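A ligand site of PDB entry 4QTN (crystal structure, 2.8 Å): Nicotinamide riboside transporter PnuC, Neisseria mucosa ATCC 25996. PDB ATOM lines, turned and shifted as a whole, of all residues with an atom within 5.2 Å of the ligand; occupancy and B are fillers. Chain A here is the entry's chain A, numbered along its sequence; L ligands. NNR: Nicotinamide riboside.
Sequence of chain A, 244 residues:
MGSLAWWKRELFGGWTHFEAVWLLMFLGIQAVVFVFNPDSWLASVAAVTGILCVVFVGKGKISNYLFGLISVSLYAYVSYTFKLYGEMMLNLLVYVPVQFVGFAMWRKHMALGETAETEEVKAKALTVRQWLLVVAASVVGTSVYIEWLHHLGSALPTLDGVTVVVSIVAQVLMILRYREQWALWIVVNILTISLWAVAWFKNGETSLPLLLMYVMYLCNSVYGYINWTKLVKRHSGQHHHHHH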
ATOM      1  N   CYS A  53       9.290   5.409 -25.681  1.00  0.00           N
ATOM      2  CA  CYS A  53       7.843   5.312 -25.604  1.00  0.00           C
ATOM      3  C   CYS A  53       7.406   5.196 -24.140  1.00  0.00           C
ATOM      4  O   CYS A  53       6.703   6.076 -23.638  1.00  0.00           O
ATOM      5  CB  CYS A  53       7.306   4.136 -26.414  1.00  0.00           C
ATOM      6  SG  CYS A  53       5.514   3.933 -26.282  1.00  0.00           S
ATOM      7  N   VAL A  54       7.846   4.140 -23.433  1.00  0.00           N
ATOM      8  CA  VAL A  54       7.219   3.841 -22.132  1.00  0.00           C
ATOM      9  C   VAL A  54       7.630   4.730 -20.982  1.00  0.00           C
ATOM     10  O   VAL A  54       6.819   5.015 -20.102  1.00  0.00           O
ATOM     11  CB  VAL A  54       7.231   2.347 -21.721  1.00  0.00           C
ATOM     12  CG1 VAL A  54       6.594   1.490 -22.797  1.00  0.00           C
ATOM     13  CG2 VAL A  54       8.629   1.861 -21.387  1.00  0.00           C
ATOM     14  N   VAL A  57       5.237   7.531 -21.691  1.00  0.00           N
ATOM     15  CA  VAL A  57       3.931   7.224 -21.080  1.00  0.00           C
ATOM     16  C   VAL A  57       3.970   7.450 -19.577  1.00  0.00           C
ATOM     17  O   VAL A  57       3.030   8.017 -18.982  1.00  0.00           O
ATOM     18  CB  VAL A  57       3.482   5.782 -21.328  1.00  0.00           C
ATOM     19  CG1 VAL A  57       2.148   5.543 -20.656  1.00  0.00           C
ATOM     20  CG2 VAL A  57       3.348   5.509 -22.813  1.00  0.00           C
ATOM     21  N   ASN A  64       5.015  10.416 -26.641  1.00  0.00           N
ATOM     22  CA  ASN A  64       5.192   9.008 -26.482  1.00  0.00           C
ATOM     23  C   ASN A  64       4.661   8.290 -27.693  1.00  0.00           C
ATOM     24  O   ASN A  64       5.168   7.226 -28.066  1.00  0.00           O
ATOM     25  CB  ASN A  64       4.514   8.500 -25.190  1.00  0.00           C
ATOM     26  CG  ASN A  64       3.013   8.275 -25.352  1.00  0.00           C
ATOM     27  OD1 ASN A  64       2.566   7.334 -26.025  1.00  0.00           O
ATOM     28  ND2 ASN A  64       2.239   9.066 -24.627  1.00  0.00           N
ATOM     29  N   GLY A  68       6.169   5.285 -29.909  1.00  0.00           N
ATOM     30  CA  GLY A  68       5.445   4.015 -29.837  1.00  0.00           C
ATOM     31  C   GLY A  68       5.205   3.416 -31.222  1.00  0.00           C
ATOM     32  O   GLY A  68       5.440   2.211 -31.462  1.00  0.00           O
ATOM     33  N   SER A  71       8.327   2.029 -32.595  1.00  0.00           N
ATOM     34  CA  SER A  71       8.671   0.913 -31.742  1.00  0.00           C
ATOM     35  C   SER A  71       7.831  -0.305 -32.033  1.00  0.00           C
ATOM     36  O   SER A  71       8.372  -1.385 -32.259  1.00  0.00           O
ATOM     37  CB  SER A  71       8.505   1.279 -30.286  1.00  0.00           C
ATOM     38  OG  SER A  71       8.762   0.158 -29.458  1.00  0.00           O
ATOM     39  N   VAL A  72       6.509  -0.145 -32.011  1.00  0.00           N
ATOM     40  CA  VAL A  72       5.617  -1.302 -32.188  1.00  0.00           C
ATOM     41  C   VAL A  72       5.704  -1.949 -33.578  1.00  0.00           C
ATOM     42  O   VAL A  72       5.425  -3.127 -33.717  1.00  0.00           O
ATOM     43  CB  VAL A  72       4.140  -0.995 -31.813  1.00  0.00           C
ATOM     44  CG1 VAL A  72       3.986  -0.871 -30.309  1.00  0.00           C
ATOM     45  CG2 VAL A  72       3.634   0.254 -32.519  1.00  0.00           C
ATOM     46  N   ASN A  91       1.015  -6.467 -31.718  1.00  0.00           N
ATOM     47  CA  ASN A  91       1.628  -5.190 -32.090  1.00  0.00           C
ATOM     48  C   ASN A  91       1.080  -4.587 -33.353  1.00  0.00           C
ATOM     49  O   ASN A  91       0.811  -3.381 -33.399  1.00  0.00           O
ATOM     50  CB  ASN A  91       3.135  -5.301 -32.151  1.00  0.00           C
ATOM     51  CG  ASN A  91       3.760  -5.233 -30.782  1.00  0.00           C
ATOM     52  OD1 ASN A  91       4.244  -4.179 -30.359  1.00  0.00           O
ATOM     53  ND2 ASN A  91       3.716  -6.341 -30.064  1.00  0.00           N
ATOM     54  N   TYR A  95      -1.766  -2.584 -31.690  1.00  0.00           N
ATOM     55  CA  TYR A  95      -0.997  -1.401 -31.241  1.00  0.00           C
ATOM     56  C   TYR A  95      -0.886  -0.260 -32.264  1.00  0.00           C
ATOM     57  O   TYR A  95      -1.039   0.919 -31.898  1.00  0.00           O
ATOM     58  CB  TYR A  95       0.388  -1.772 -30.632  1.00  0.00           C
ATOM     59  CG  TYR A  95       0.326  -2.496 -29.269  1.00  0.00           C
ATOM     60  CD1 TYR A  95      -0.821  -2.465 -28.472  1.00  0.00           C
ATOM     61  CD2 TYR A  95       1.421  -3.206 -28.786  1.00  0.00           C
ATOM     62  CE1 TYR A  95      -0.880  -3.126 -27.264  1.00  0.00           C
ATOM     63  CE2 TYR A  95       1.369  -3.883 -27.579  1.00  0.00           C
ATOM     64  CZ  TYR A  95       0.220  -3.826 -26.820  1.00  0.00           C
ATOM     65  OH  TYR A  95       0.162  -4.480 -25.628  1.00  0.00           O
ATOM     66  N   GLN A  99      -1.869   3.669 -31.400  1.00  0.00           N
ATOM     67  CA  GLN A  99      -0.995   4.830 -31.380  1.00  0.00           C
ATOM     68  C   GLN A  99      -1.714   6.051 -31.937  1.00  0.00           C
ATOM     69  O   GLN A  99      -1.511   7.171 -31.473  1.00  0.00           O
ATOM     70  CB  GLN A  99       0.286   4.586 -32.161  1.00  0.00           C
ATOM     71  CG  GLN A  99       1.228   3.547 -31.548  1.00  0.00           C
ATOM     72  CD  GLN A  99       1.454   3.754 -30.071  1.00  0.00           C
ATOM     73  OE1 GLN A  99       2.084   4.738 -29.642  1.00  0.00           O
ATOM     74  NE2 GLN A  99       0.942   2.831 -29.265  1.00  0.00           N
ATOM     75  N   GLN A 171      -3.766  -1.552 -22.426  1.00  0.00           N
ATOM     76  CA  GLN A 171      -3.772  -0.480 -23.430  1.00  0.00           C
ATOM     77  C   GLN A 171      -5.106   0.308 -23.515  1.00  0.00           C
ATOM     78  O   GLN A 171      -5.087   1.502 -23.788  1.00  0.00           O
ATOM     79  CB  GLN A 171      -3.341  -0.986 -24.797  1.00  0.00           C
ATOM     80  CG  GLN A 171      -2.958   0.138 -25.745  1.00  0.00           C
ATOM     81  CD  GLN A 171      -1.468   0.402 -25.770  1.00  0.00           C
ATOM     82  OE1 GLN A 171      -0.684  -0.474 -26.126  1.00  0.00           O
ATOM     83  NE2 GLN A 171      -1.078   1.601 -25.407  1.00  0.00           N
ATOM     84  N   MET A 174      -4.817   2.684 -20.605  1.00  0.00           N
ATOM     85  CA  MET A 174      -3.907   3.754 -20.937  1.00  0.00           C
ATOM     86  C   MET A 174      -4.608   4.821 -21.722  1.00  0.00           C
ATOM     87  O   MET A 174      -4.530   6.005 -21.374  1.00  0.00           O
ATOM     88  CB  MET A 174      -2.730   3.252 -21.751  1.00  0.00           C
ATOM     89  CG  MET A 174      -1.667   4.327 -21.782  1.00  0.00           C
ATOM     90  SD  MET A 174      -0.901   4.376 -23.584  1.00  0.00           S
ATOM     91  CE  MET A 174      -0.087   6.168 -23.635  1.00  0.00           C
ATOM     92  N   GLN A 181      -3.691   1.203 -15.236  1.00  0.00           N
ATOM     93  CA  GLN A 181      -2.991   0.565 -16.346  1.00  0.00           C
ATOM     94  C   GLN A 181      -1.687  -0.056 -15.875  1.00  0.00           C
ATOM     95  O   GLN A 181      -1.376  -1.192 -16.226  1.00  0.00           O
ATOM     96  CB  GLN A 181      -2.720   1.552 -17.470  1.00  0.00           C
ATOM     97  CG  GLN A 181      -2.024   2.791 -17.011  1.00  0.00           C
ATOM     98  CD  GLN A 181      -1.361   3.532 -18.127  1.00  0.00           C
ATOM     99  OE1 GLN A 181      -0.659   2.933 -18.952  1.00  0.00           O
ATOM    100  NE2 GLN A 181      -1.522   4.847 -18.157  1.00  0.00           N
ATOM    101  N   TRP A 182      -0.936   0.665 -15.065  1.00  0.00           N
ATOM    102  CA  TRP A 182       0.380   0.185 -14.662  1.00  0.00           C
ATOM    103  C   TRP A 182       0.405  -1.117 -13.858  1.00  0.00           C
ATOM    104  O   TRP A 182       1.393  -1.829 -13.876  1.00  0.00           O
ATOM    105  CB  TRP A 182       1.154   1.259 -13.944  1.00  0.00           C
ATOM    106  CG  TRP A 182       1.320   2.454 -14.737  1.00  0.00           C
ATOM    107  CD1 TRP A 182       0.611   3.616 -14.609  1.00  0.00           C
ATOM    108  CD2 TRP A 182       2.241   2.662 -15.792  1.00  0.00           C
ATOM    109  NE1 TRP A 182       1.064   4.547 -15.508  1.00  0.00           N
ATOM    110  CE2 TRP A 182       2.067   3.987 -16.250  1.00  0.00           C
ATOM    111  CE3 TRP A 182       3.222   1.860 -16.379  1.00  0.00           C
ATOM    112  CZ2 TRP A 182       2.835   4.525 -17.282  1.00  0.00           C
ATOM    113  CZ3 TRP A 182       3.973   2.397 -17.406  1.00  0.00           C
ATOM    114  CH2 TRP A 182       3.772   3.729 -17.856  1.00  0.00           C
ATOM    115  N   TRP A 185       0.366  -3.490 -16.799  1.00  0.00           N
ATOM    116  CA  TRP A 185       1.657  -3.464 -17.475  1.00  0.00           C
ATOM    117  C   TRP A 185       2.701  -4.257 -16.701  1.00  0.00           C
ATOM    118  O   TRP A 185       3.549  -4.939 -17.302  1.00  0.00           O
ATOM    119  CB  TRP A 185       2.150  -2.037 -17.676  1.00  0.00           C
ATOM    120  CG  TRP A 185       1.298  -1.207 -18.564  1.00  0.00           C
ATOM    121  CD1 TRP A 185       0.761   0.009 -18.263  1.00  0.00           C
ATOM    122  CD2 TRP A 185       0.917  -1.491 -19.913  1.00  0.00           C
ATOM    123  NE1 TRP A 185       0.066   0.499 -19.337  1.00  0.00           N
ATOM    124  CE2 TRP A 185       0.145  -0.411 -20.359  1.00  0.00           C
ATOM    125  CE3 TRP A 185       1.144  -2.563 -20.779  1.00  0.00           C
ATOM    126  CZ2 TRP A 185      -0.406  -0.368 -21.642  1.00  0.00           C
ATOM    127  CZ3 TRP A 185       0.610  -2.513 -22.046  1.00  0.00           C
ATOM    128  CH2 TRP A 185      -0.161  -1.415 -22.464  1.00  0.00           C
ATOM    129  N   VAL A 188       2.076  -7.784 -17.694  1.00  0.00           N
ATOM    130  CA  VAL A 188       2.506  -8.070 -19.081  1.00  0.00           C
ATOM    131  C   VAL A 188       4.033  -8.003 -19.276  1.00  0.00           C
ATOM    132  O   VAL A 188       4.594  -8.764 -20.080  1.00  0.00           O
ATOM    133  CB  VAL A 188       1.732  -7.262 -20.191  1.00  0.00           C
ATOM    134  CG1 VAL A 188       0.406  -6.763 -19.665  1.00  0.00           C
ATOM    135  CG2 VAL A 188       2.552  -6.121 -20.762  1.00  0.00           C
ATOM    136  N   ASN A 189       4.708  -7.130 -18.546  1.00  0.00           N
ATOM    137  CA  ASN A 189       6.147  -7.043 -18.635  1.00  0.00           C
ATOM    138  C   ASN A 189       6.822  -8.284 -18.026  1.00  0.00           C
ATOM    139  O   ASN A 189       7.860  -8.745 -18.498  1.00  0.00           O
ATOM    140  CB  ASN A 189       6.656  -5.766 -17.989  1.00  0.00           C
ATOM    141  CG  ASN A 189       6.493  -4.552 -18.884  1.00  0.00           C
ATOM    142  OD1 ASN A 189       6.364  -3.424 -18.394  1.00  0.00           O
ATOM    143  ND2 ASN A 189       6.503  -4.764 -20.188  1.00  0.00           N
ATOM    144  N   TYR A 214      12.409  -5.396 -22.336  1.00  0.00           N
ATOM    145  CA  TYR A 214      11.340  -5.814 -21.409  1.00  0.00           C
ATOM    146  C   TYR A 214      11.739  -5.887 -19.898  1.00  0.00           C
ATOM    147  O   TYR A 214      10.875  -5.750 -19.025  1.00  0.00           O
ATOM    148  CB  TYR A 214      10.666  -7.093 -21.885  1.00  0.00           C
ATOM    149  CG  TYR A 214       9.571  -6.811 -22.863  1.00  0.00           C
ATOM    150  CD1 TYR A 214       8.322  -6.383 -22.435  1.00  0.00           C
ATOM    151  CD2 TYR A 214       9.800  -6.907 -24.237  1.00  0.00           C
ATOM    152  CE1 TYR A 214       7.306  -6.089 -23.334  1.00  0.00           C
ATOM    153  CE2 TYR A 214       8.792  -6.621 -25.152  1.00  0.00           C
ATOM    154  CZ  TYR A 214       7.541  -6.208 -24.693  1.00  0.00           C
ATOM    155  OH  TYR A 214       6.532  -5.930 -25.592  1.00  0.00           O
ATOM    156  N   TYR A 217      11.534  -2.287 -19.305  1.00  0.00           N
ATOM    157  CA  TYR A 217      10.094  -2.017 -19.212  1.00  0.00           C
ATOM    158  C   TYR A 217       9.562  -2.239 -17.821  1.00  0.00           C
ATOM    159  O   TYR A 217       8.758  -1.434 -17.326  1.00  0.00           O
ATOM    160  CB  TYR A 217       9.282  -2.838 -20.217  1.00  0.00           C
ATOM    161  CG  TYR A 217       9.148  -2.199 -21.564  1.00  0.00           C
ATOM    162  CD1 TYR A 217      10.054  -1.227 -22.005  1.00  0.00           C
ATOM    163  CD2 TYR A 217       8.153  -2.607 -22.434  1.00  0.00           C
ATOM    164  CE1 TYR A 217       9.957  -0.669 -23.267  1.00  0.00           C
ATOM    165  CE2 TYR A 217       8.036  -2.051 -23.704  1.00  0.00           C
ATOM    166  CZ  TYR A 217       8.938  -1.082 -24.120  1.00  0.00           C
ATOM    167  OH  TYR A 217       8.812  -0.523 -25.396  1.00  0.00           O
ATOM    168  N   ASN A 220      10.547   0.411 -15.445  1.00  0.00           N
ATOM    169  CA  ASN A 220       9.818   1.635 -15.702  1.00  0.00           C
ATOM    170  C   ASN A 220       8.336   1.534 -15.406  1.00  0.00           C
ATOM    171  O   ASN A 220       7.729   2.522 -15.003  1.00  0.00           O
ATOM    172  CB  ASN A 220      10.066   2.133 -17.115  1.00  0.00           C
ATOM    173  CG  ASN A 220       9.039   3.160 -17.553  1.00  0.00           C
ATOM    174  OD1 ASN A 220       9.245   4.381 -17.410  1.00  0.00           O
ATOM    175  ND2 ASN A 220       7.912   2.677 -18.100  1.00  0.00           N
ATOM    176  N   SER A 221       7.756   0.339 -15.541  1.00  0.00           N
ATOM    177  CA  SER A 221       6.332   0.157 -15.248  1.00  0.00           C
ATOM    178  C   SER A 221       5.995   0.347 -13.754  1.00  0.00           C
ATOM    179  O   SER A 221       4.878   0.690 -13.403  1.00  0.00           O
ATOM    180  CB  SER A 221       5.812  -1.186 -15.766  1.00  0.00           C
ATOM    181  OG  SER A 221       6.225  -2.258 -14.952  1.00  0.00           O
HETATM  182  O2R NNR L   1       1.819   2.811 -25.649  1.00  0.00           O
HETATM  183  C2R NNR L   1       2.699   1.587 -25.334  1.00  0.00           C
HETATM  184  C3R NNR L   1       3.059   0.878 -26.638  1.00  0.00           C
HETATM  185  O3R NNR L   1       1.962   0.807 -27.441  1.00  0.00           O
HETATM  186  C4R NNR L   1       3.424  -0.510 -26.181  1.00  0.00           C
HETATM  187  C5R NNR L   1       4.942  -0.540 -25.741  1.00  0.00           C
HETATM  188  O5R NNR L   1       5.556  -1.821 -26.119  1.00  0.00           O
HETATM  189  O4R NNR L   1       2.601  -0.781 -25.194  1.00  0.00           O
HETATM  190  C1R NNR L   1       2.120   0.651 -24.589  1.00  0.00           C
HETATM  191  N1  NNR L   1       2.534   0.745 -23.173  1.00  0.00           N
HETATM  192  C2  NNR L   1       3.323  -0.226 -22.594  1.00  0.00           C
HETATM  193  C6  NNR L   1       2.153   1.830 -22.409  1.00  0.00           C
HETATM  194  C5  NNR L   1       2.566   1.952 -21.070  1.00  0.00           C
HETATM  195  C4  NNR L   1       3.339   0.994 -20.517  1.00  0.00           C
HETATM  196  C3  NNR L   1       3.733  -0.080 -21.256  1.00  0.00           C
HETATM  197  C7  NNR L   1       4.607  -1.149 -20.597  1.00  0.00           C
HETATM  198  O7  NNR L   1       4.392  -2.298 -20.795  1.00  0.00           O
HETATM  199  N7  NNR L   1       5.703  -0.760 -19.757  1.00  0.00           N
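O3R of the ligand lies within hydrogen-bond range of NE2 of Gln 99 (2.9 Å). A nitrogen (N7) of the ligand sits at hydrogen-bond distance from the side-chain amide oxygen of Asn 189 (3.1 Å). An oxygen (O2R) of the ligand is in hydrogen-bond range of the side-chain amide nitrogen (NE2) of Gln 171, at 3.1 Å. The side-chain sulfur (SD) of Met 174 is in hydrogen-bond range of an oxygen (O2R) of the ligand (3.8 Å).
The side-chain amide oxygen of Asn 189 sits close to the backbone carbonyl oxygen of Trp 185, 3.4 Å away. The side-chain amide oxygen (OD1) of Asn 189 lies close to the backbone carbonyl oxygen (O) of Tyr 217, at 3.3 Å. NE2 of Gln 171 is in hydrogen-bond range of SD of Met 174 (3.3 Å). The indole nitrogen of Trp 185 lies within hydrogen-bond range of the side-chain amide oxygen of Gln 181, 2.6 Å away. The backbone carbonyl oxygen of Val 54 lies within hydrogen-bond range of the side-chain amide nitrogen of Asn 220 (3.3 Å). The side-chain sulfur of Cys 53 lies within hydrogen-bond range of the backbone carbonyl oxygen of Asn 64, 3.8 Å away.
Residues that only touch the ligand: Cys 53 (3.8 Å), Val 54 (3.6 Å), Val 57 (3.6 Å), Val 72 (3.9 Å), Gln 181 (3.98 Å), Trp 182 (3.5 Å), Trp 185 (3.3 Å) and Tyr 217 (3.5 Å). Hydrophobic or aromatic side chains within 4 Å of the ligand: Val 54, Val 57, Val 72, Met 174, Trp 182, Trp 185 and Tyr 217. 12 residues have an atom within 4 Å of the ligand: Cys 53, Val 54, Val 57, Val 72, Gln 99, Gln 171, Met 174, Gln 181, Trp 182, Trp 185, Asn 189 and Tyr 217. The nearest printed residue that does not touch the ligand is Ser 221 (4.02 Å).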
